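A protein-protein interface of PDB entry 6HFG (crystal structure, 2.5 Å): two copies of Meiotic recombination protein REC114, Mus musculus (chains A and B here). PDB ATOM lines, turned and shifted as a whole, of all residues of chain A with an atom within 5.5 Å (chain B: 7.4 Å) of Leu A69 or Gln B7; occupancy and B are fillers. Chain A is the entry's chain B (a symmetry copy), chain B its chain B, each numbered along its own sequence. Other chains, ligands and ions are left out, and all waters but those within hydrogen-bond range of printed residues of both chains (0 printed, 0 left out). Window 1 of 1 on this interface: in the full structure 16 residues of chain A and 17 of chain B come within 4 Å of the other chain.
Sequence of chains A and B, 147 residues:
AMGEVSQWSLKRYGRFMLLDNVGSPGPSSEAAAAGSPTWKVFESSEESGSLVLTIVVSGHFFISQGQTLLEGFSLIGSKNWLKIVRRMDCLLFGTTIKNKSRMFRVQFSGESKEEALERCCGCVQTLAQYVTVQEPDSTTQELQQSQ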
ATOM      1  N   PHE A  62      21.211  -1.794  21.017  1.00  0.00           N
ATOM      2  CA  PHE A  62      20.541  -0.636  21.537  1.00  0.00           C
ATOM      3  C   PHE A  62      21.473   0.571  21.505  1.00  0.00           C
ATOM      4  O   PHE A  62      22.707   0.435  21.652  1.00  0.00           O
ATOM      5  CB  PHE A  62      20.100  -0.864  22.978  1.00  0.00           C
ATOM      6  CG  PHE A  62      19.180  -2.039  23.157  1.00  0.00           C
ATOM      7  CD1 PHE A  62      17.826  -1.907  22.921  1.00  0.00           C
ATOM      8  CD2 PHE A  62      19.672  -3.267  23.543  1.00  0.00           C
ATOM      9  CE1 PHE A  62      16.987  -2.993  23.060  1.00  0.00           C
ATOM     10  CE2 PHE A  62      18.828  -4.347  23.696  1.00  0.00           C
ATOM     11  CZ  PHE A  62      17.490  -4.212  23.449  1.00  0.00           C
ATOM     12  N   ILE A  63      20.853   1.735  21.318  1.00  0.00           N
ATOM     13  CA  ILE A  63      21.433   3.005  21.692  1.00  0.00           C
ATOM     14  C   ILE A  63      20.526   3.628  22.747  1.00  0.00           C
ATOM     15  O   ILE A  63      19.304   3.627  22.609  1.00  0.00           O
ATOM     16  CB  ILE A  63      21.592   3.927  20.480  1.00  0.00           C
ATOM     17  CG1 ILE A  63      22.656   3.390  19.527  1.00  0.00           C
ATOM     18  CG2 ILE A  63      21.896   5.347  20.933  1.00  0.00           C
ATOM     19  CD1 ILE A  63      22.447   3.835  18.119  1.00  0.00           C
ATOM     20  N   SER A  64      21.139   4.144  23.806  1.00  0.00           N
ATOM     21  CA  SER A  64      20.379   4.736  24.852  1.00  0.00           C
ATOM     22  C   SER A  64      21.063   6.023  25.308  1.00  0.00           C
ATOM     23  O   SER A  64      22.274   6.134  25.271  1.00  0.00           O
ATOM     24  CB  SER A  64      20.157   3.754  25.973  1.00  0.00           C
ATOM     25  OG  SER A  64      21.376   3.390  26.587  1.00  0.00           O
ATOM     26  N   GLN A  65      20.232   7.000  25.679  1.00  0.00           N
ATOM     27  CA  GLN A  65      20.635   8.251  26.292  1.00  0.00           C
ATOM     28  C   GLN A  65      19.996   8.289  27.682  1.00  0.00           C
ATOM     29  O   GLN A  65      18.761   8.333  27.815  1.00  0.00           O
ATOM     30  CB  GLN A  65      20.183   9.416  25.415  1.00  0.00           C
ATOM     31  CG  GLN A  65      20.709  10.779  25.843  1.00  0.00           C
ATOM     32  CD  GLN A  65      20.037  11.870  25.043  1.00  0.00           C
ATOM     33  OE1 GLN A  65      18.804  11.933  24.937  1.00  0.00           O
ATOM     34  NE2 GLN A  65      20.854  12.742  24.466  1.00  0.00           N
ATOM     35  N   GLN A  67      18.319   6.690  30.151  1.00  0.00           N
ATOM     36  CA  GLN A  67      17.466   5.526  30.321  1.00  0.00           C
ATOM     37  C   GLN A  67      16.441   5.410  29.187  1.00  0.00           C
ATOM     38  O   GLN A  67      15.777   4.375  29.085  1.00  0.00           O
ATOM     39  CB  GLN A  67      16.814   5.586  31.702  1.00  0.00           C
ATOM     40  CG  GLN A  67      17.847   5.581  32.822  1.00  0.00           C
ATOM     41  CD  GLN A  67      17.292   5.005  34.101  1.00  0.00           C
ATOM     42  OE1 GLN A  67      16.173   5.324  34.502  1.00  0.00           O
ATOM     43  NE2 GLN A  67      18.066   4.133  34.733  1.00  0.00           N
ATOM     44  N   THR A  68      16.345   6.435  28.327  1.00  0.00           N
ATOM     45  CA  THR A  68      15.500   6.356  27.132  1.00  0.00           C
ATOM     46  C   THR A  68      16.252   5.544  26.062  1.00  0.00           C
ATOM     47  O   THR A  68      17.455   5.700  25.868  1.00  0.00           O
ATOM     48  CB  THR A  68      15.041   7.743  26.649  1.00  0.00           C
ATOM     49  OG1 THR A  68      15.975   8.217  25.686  1.00  0.00           O
ATOM     50  CG2 THR A  68      14.894   8.765  27.759  1.00  0.00           C
ATOM     51  N   LEU A  69      15.529   4.634  25.409  1.00  0.00           N
ATOM     52  CA  LEU A  69      16.050   3.814  24.344  1.00  0.00           C
ATOM     53  C   LEU A  69      15.710   4.487  23.013  1.00  0.00           C
ATOM     54  O   LEU A  69      14.548   4.608  22.643  1.00  0.00           O
ATOM     55  CB  LEU A  69      15.436   2.414  24.420  1.00  0.00           C
ATOM     56  CG  LEU A  69      15.883   1.549  25.590  1.00  0.00           C
ATOM     57  CD1 LEU A  69      15.160   0.215  25.550  1.00  0.00           C
ATOM     58  CD2 LEU A  69      17.388   1.334  25.579  1.00  0.00           C
ATOM     59  N   LEU A  70      16.757   4.928  22.319  1.00  0.00           N
ATOM     60  CA  LEU A  70      16.646   5.618  21.077  1.00  0.00           C
ATOM     61  C   LEU A  70      16.613   4.613  19.925  1.00  0.00           C
ATOM     62  O   LEU A  70      16.101   4.906  18.868  1.00  0.00           O
ATOM     63  CB  LEU A  70      17.846   6.558  20.959  1.00  0.00           C
ATOM     64  CG  LEU A  70      17.971   7.595  22.074  1.00  0.00           C
ATOM     65  CD1 LEU A  70      19.186   8.484  21.837  1.00  0.00           C
ATOM     66  CD2 LEU A  70      16.708   8.445  22.176  1.00  0.00           C
ATOM     67  N   GLU A  71      17.198   3.434  20.122  1.00  0.00           N
ATOM     68  CA  GLU A  71      17.262   2.462  19.054  1.00  0.00           C
ATOM     69  C   GLU A  71      17.276   1.076  19.690  1.00  0.00           C
ATOM     70  O   GLU A  71      17.841   0.906  20.765  1.00  0.00           O
ATOM     71  CB  GLU A  71      18.485   2.733  18.170  1.00  0.00           C
ATOM     72  CG  GLU A  71      18.221   2.498  16.695  1.00  0.00           C
ATOM     73  CD  GLU A  71      17.596   3.649  15.925  1.00  0.00           C
ATOM     74  OE1 GLU A  71      17.753   4.811  16.336  1.00  0.00           O
ATOM     75  OE2 GLU A  71      16.960   3.375  14.896  1.00  0.00           O
ATOM     76  N   ALA B   1      10.919   0.841  26.185  1.00  0.00           N
ATOM     77  CA  ALA B   1      10.415   1.737  25.095  1.00  0.00           C
ATOM     78  C   ALA B   1       9.994   0.914  23.858  1.00  0.00           C
ATOM     79  O   ALA B   1       8.830   0.959  23.444  1.00  0.00           O
ATOM     80  CB  ALA B   1      11.468   2.774  24.771  1.00  0.00           C
ATOM     81  N   MET B   2      10.941   0.146  23.297  1.00  0.00           N
ATOM     82  CA  MET B   2      10.809  -0.586  22.009  1.00  0.00           C
ATOM     83  C   MET B   2       9.811  -1.754  22.123  1.00  0.00           C
ATOM     84  O   MET B   2       9.205  -1.958  23.172  1.00  0.00           O
ATOM     85  CB  MET B   2      12.181  -1.128  21.580  1.00  0.00           C
ATOM     86  CG  MET B   2      13.117  -0.062  21.041  1.00  0.00           C
ATOM     87  SD  MET B   2      12.434   0.834  19.610  1.00  0.00           S
ATOM     88  CE  MET B   2      11.836  -0.498  18.568  1.00  0.00           C
ATOM     89  N   GLU B   4      11.149  -4.632  21.513  1.00  0.00           N
ATOM     90  CA  GLU B   4      12.250  -5.560  21.613  1.00  0.00           C
ATOM     91  C   GLU B   4      12.617  -5.775  23.085  1.00  0.00           C
ATOM     92  O   GLU B   4      13.420  -6.637  23.425  1.00  0.00           O
ATOM     93  CB  GLU B   4      13.406  -4.970  20.810  1.00  0.00           C
ATOM     94  CG  GLU B   4      13.318  -5.354  19.349  1.00  0.00           C
ATOM     95  CD  GLU B   4      13.937  -6.714  19.123  1.00  0.00           C
ATOM     96  OE1 GLU B   4      13.330  -7.534  18.391  1.00  0.00           O
ATOM     97  OE2 GLU B   4      15.036  -6.941  19.703  1.00  0.00           O
ATOM     98  N   VAL B   5      11.995  -4.974  23.947  1.00  0.00           N
ATOM     99  CA  VAL B   5      12.307  -4.905  25.338  1.00  0.00           C
ATOM    100  C   VAL B   5      11.014  -4.626  26.098  1.00  0.00           C
ATOM    101  O   VAL B   5      10.104  -4.018  25.572  1.00  0.00           O
ATOM    102  CB  VAL B   5      13.355  -3.812  25.595  1.00  0.00           C
ATOM    103  CG1 VAL B   5      13.605  -3.587  27.063  1.00  0.00           C
ATOM    104  CG2 VAL B   5      14.649  -4.165  24.914  1.00  0.00           C
ATOM    105  N   SER B   6      10.947  -5.127  27.326  1.00  0.00           N
ATOM    106  CA  SER B   6      10.017  -4.629  28.327  1.00  0.00           C
ATOM    107  C   SER B   6      10.831  -4.049  29.490  1.00  0.00           C
ATOM    108  O   SER B   6      11.921  -4.541  29.814  1.00  0.00           O
ATOM    109  CB  SER B   6       9.079  -5.715  28.768  1.00  0.00           C
ATOM    110  OG  SER B   6       8.286  -6.152  27.679  1.00  0.00           O
ATOM    111  N   GLN B   7      10.313  -2.978  30.086  1.00  0.00           N
ATOM    112  CA  GLN B   7      11.005  -2.294  31.157  1.00  0.00           C
ATOM    113  C   GLN B   7      10.011  -1.912  32.244  1.00  0.00           C
ATOM    114  O   GLN B   7       8.879  -1.575  31.954  1.00  0.00           O
ATOM    115  CB  GLN B   7      11.723  -1.058  30.627  1.00  0.00           C
ATOM    116  CG  GLN B   7      12.945  -1.406  29.788  1.00  0.00           C
ATOM    117  CD  GLN B   7      13.709  -0.171  29.383  1.00  0.00           C
ATOM    118  OE1 GLN B   7      13.153   0.719  28.736  1.00  0.00           O
ATOM    119  NE2 GLN B   7      14.977  -0.108  29.775  1.00  0.00           N
ATOM    120  N   TRP B   8      10.474  -1.989  33.491  1.00  0.00           N
ATOM    121  CA  TRP B   8       9.706  -1.637  34.692  1.00  0.00           C
ATOM    122  C   TRP B   8      10.641  -0.873  35.605  1.00  0.00           C
ATOM    123  O   TRP B   8      11.815  -1.273  35.744  1.00  0.00           O
ATOM    124  CB  TRP B   8       9.200  -2.880  35.440  1.00  0.00           C
ATOM    125  CG  TRP B   8       8.326  -3.773  34.624  1.00  0.00           C
ATOM    126  CD1 TRP B   8       6.964  -3.766  34.588  1.00  0.00           C
ATOM    127  CD2 TRP B   8       8.752  -4.790  33.701  1.00  0.00           C
ATOM    128  NE1 TRP B   8       6.514  -4.718  33.717  1.00  0.00           N
ATOM    129  CE2 TRP B   8       7.582  -5.364  33.156  1.00  0.00           C
ATOM    130  CE3 TRP B   8       9.996  -5.271  33.281  1.00  0.00           C
ATOM    131  CZ2 TRP B   8       7.622  -6.398  32.220  1.00  0.00           C
ATOM    132  CZ3 TRP B   8      10.040  -6.293  32.354  1.00  0.00           C
ATOM    133  CH2 TRP B   8       8.866  -6.850  31.836  1.00  0.00           C
ATOM    134  N   SER B   9      10.115   0.159  36.261  1.00  0.00           N
ATOM    135  CA  SER B   9      10.929   0.902  37.193  1.00  0.00           C
ATOM    136  C   SER B   9      10.805   0.280  38.590  1.00  0.00           C
ATOM    137  O   SER B   9       9.741  -0.218  38.967  1.00  0.00           O
ATOM    138  CB  SER B   9      10.580   2.367  37.170  1.00  0.00           C
ATOM    139  OG  SER B   9       9.343   2.575  37.795  1.00  0.00           O
ATOM    140  N   VAL B  52      15.863   0.467  36.891  1.00  0.00           N
ATOM    141  CA  VAL B  52      15.115  -0.080  35.818  1.00  0.00           C
ATOM    142  C   VAL B  52      15.471  -1.558  35.729  1.00  0.00           C
ATOM    143  O   VAL B  52      16.661  -1.906  35.793  1.00  0.00           O
ATOM    144  CB  VAL B  52      15.442   0.661  34.513  1.00  0.00           C
ATOM    145  CG1 VAL B  52      14.702   0.075  33.322  1.00  0.00           C
ATOM    146  CG2 VAL B  52      15.142   2.139  34.662  1.00  0.00           C
ATOM    147  N   LEU B  53      14.429  -2.396  35.628  1.00  0.00           N
ATOM    148  CA  LEU B  53      14.551  -3.818  35.328  1.00  0.00           C
ATOM    149  C   LEU B  53      14.132  -3.995  33.875  1.00  0.00           C
ATOM    150  O   LEU B  53      13.047  -3.560  33.482  1.00  0.00           O
ATOM    151  CB  LEU B  53      13.649  -4.619  36.269  1.00  0.00           C
ATOM    152  CG  LEU B  53      13.792  -6.144  36.226  1.00  0.00           C
ATOM    153  CD1 LEU B  53      13.167  -6.775  37.464  1.00  0.00           C
ATOM    154  CD2 LEU B  53      13.177  -6.736  34.963  1.00  0.00           C
ATOM    155  N   THR B  54      15.008  -4.621  33.092  1.00  0.00           N
ATOM    156  CA  THR B  54      14.823  -4.718  31.665  1.00  0.00           C
ATOM    157  C   THR B  54      14.828  -6.193  31.287  1.00  0.00           C
ATOM    158  O   THR B  54      15.723  -6.931  31.699  1.00  0.00           O
ATOM    159  CB  THR B  54      15.940  -3.999  30.889  1.00  0.00           C
ATOM    160  OG1 THR B  54      15.949  -2.605  31.187  1.00  0.00           O
ATOM    161  CG2 THR B  54      15.780  -4.127  29.391  1.00  0.00           C
ATOM    162  N   ILE B  55      13.843  -6.605  30.491  1.00  0.00           N
ATOM    163  CA  ILE B  55      13.886  -7.914  29.907  1.00  0.00           C
ATOM    164  C   ILE B  55      13.791  -7.763  28.395  1.00  0.00           C
ATOM    165  O   ILE B  55      12.819  -7.231  27.879  1.00  0.00           O
ATOM    166  CB  ILE B  55      12.803  -8.862  30.463  1.00  0.00           C
ATOM    167  CG1 ILE B  55      12.961  -9.080  31.969  1.00  0.00           C
ATOM    168  CG2 ILE B  55      12.859 -10.178  29.714  1.00  0.00           C
ATOM    169  CD1 ILE B  55      11.781  -9.755  32.635  1.00  0.00           C
ATOM    170  N   VAL B  56      14.814  -8.282  27.726  1.00  0.00           N
ATOM    171  CA  VAL B  56      14.958  -8.257  26.303  1.00  0.00           C
ATOM    172  C   VAL B  56      14.317  -9.533  25.753  1.00  0.00           C
ATOM    173  O   VAL B  56      14.408 -10.572  26.371  1.00  0.00           O
ATOM    174  CB  VAL B  56      16.445  -8.163  25.919  1.00  0.00           C
ATOM    175  CG1 VAL B  56      16.626  -7.981  24.423  1.00  0.00           C
ATOM    176  CG2 VAL B  56      17.158  -7.068  26.689  1.00  0.00           C
ATOM    177  N   SER B  64      19.444  -1.921  35.965  1.00  0.00           N
ATOM    178  CA  SER B  64      20.363  -0.854  35.769  1.00  0.00           C
ATOM    179  C   SER B  64      19.921   0.353  36.591  1.00  0.00           C
ATOM    180  O   SER B  64      18.742   0.571  36.797  1.00  0.00           O
ATOM    181  CB  SER B  64      20.521  -0.548  34.302  1.00  0.00           C
ATOM    182  OG  SER B  64      19.312  -0.077  33.743  1.00  0.00           O
ATOM    183  N   PHE B 108       9.323  -3.160  43.029  1.00  0.00           N
ATOM    184  CA  PHE B 108       8.787  -2.336  41.962  1.00  0.00           C
ATOM    185  C   PHE B 108       8.215  -1.060  42.570  1.00  0.00           C
ATOM    186  O   PHE B 108       7.790  -1.072  43.707  1.00  0.00           O
ATOM    187  CB  PHE B 108       7.725  -3.094  41.158  1.00  0.00           C
ATOM    188  CG  PHE B 108       8.279  -4.269  40.395  1.00  0.00           C
ATOM    189  CD1 PHE B 108       8.671  -4.140  39.079  1.00  0.00           C
ATOM    190  CD2 PHE B 108       8.453  -5.498  41.006  1.00  0.00           C
ATOM    191  CE1 PHE B 108       9.210  -5.213  38.387  1.00  0.00           C
ATOM    192  CE2 PHE B 108       8.982  -6.574  40.307  1.00  0.00           C
ATOM    193  CZ  PHE B 108       9.373  -6.425  39.001  1.00  0.00           C
ATOM    194  N   ARG B 119       2.654  -3.322  38.483  1.00  0.00           N
ATOM    195  CA  ARG B 119       3.939  -3.340  37.819  1.00  0.00           C
ATOM    196  C   ARG B 119       4.584  -4.718  37.986  1.00  0.00           C
ATOM    197  O   ARG B 119       4.912  -5.373  37.000  1.00  0.00           O
ATOM    198  CB  ARG B 119       4.890  -2.297  38.410  1.00  0.00           C
ATOM    199  CG  ARG B 119       4.890  -0.968  37.683  1.00  0.00           C
ATOM    200  CD  ARG B 119       6.078  -0.114  38.081  1.00  0.00           C
ATOM    201  NE  ARG B 119       5.857   1.210  37.525  1.00  0.00           N
ATOM    202  CZ  ARG B 119       4.812   1.983  37.814  1.00  0.00           C
ATOM    203  NH1 ARG B 119       4.276   1.970  39.022  1.00  0.00           N
ATOM    204  NH2 ARG B 119       4.286   2.737  36.871  1.00  0.00           N
ATOM    205  N   CYS B 123       5.612  -7.856  35.144  1.00  0.00           N
ATOM    206  CA  CYS B 123       6.948  -8.336  35.003  1.00  0.00           C
ATOM    207  C   CYS B 123       6.954  -9.852  35.217  1.00  0.00           C
ATOM    208  O   CYS B 123       7.597 -10.596  34.476  1.00  0.00           O
ATOM    209  CB  CYS B 123       7.864  -7.609  35.977  1.00  0.00           C
ATOM    210  SG  CYS B 123       9.586  -8.161  35.918  1.00  0.00           S
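The backbone NH of Ser B64 lies within hydrogen-bond range of the backbone carbonyl oxygen of Val B52, 2.8 Å away.
OE1 of Gln B7 is in hydrogen-bond range of N of Ala B1 (3.4 Å).
NE2 of Gln B7 lies within hydrogen-bond range of OG1 of Thr B54 (3.0 Å).
CZ of Phe A62 touches CG2 of Val B5 (3.2 Å).
CZ of Phe A62 touches CG1 of Val B56, 3.99 Å away.
Gln A67 touches Val B52 (OE1 to CG2, 3.4 Å).
Ala B1 touches Leu A69 (CB to CB, 3.9997 Å).
Leu A69 touches Gln B7.
Gln B7 touches just one residue of chain A: Leu A69.
Printed residues of chain B within 4 Å of Gln A67: Val B52.
Of the printed residues of chain A, Ala B1 touches Leu A69.
Of the printed residues of chain A, Val B56 touches Phe A62 (3.99 Å).
Printed residues of chain A within 4 Å of Val B52: Gln A67.
Gln A65 touches none of the printed residues of chain B.
The nearest printed residue of chain B that does not touch Leu A69 is Val B5 (4.4 Å).
Printed residues of chain A that touch a printed residue of chain B: Phe A62, Gln A67 and Leu A69.
Hydrophobic or aromatic side chains of chain B within 4 Å of the printed part of chain A: Ala B1, Val B5, Val B52 and Val B56.
Along chain B the printed residues that touch a printed residue of chain A span positions 1 to 56.
Position printed for both chains: 64.
Of the 5 pairs that touch across the chains among the printed residues, none has its exchanged pair printed and touching as well.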
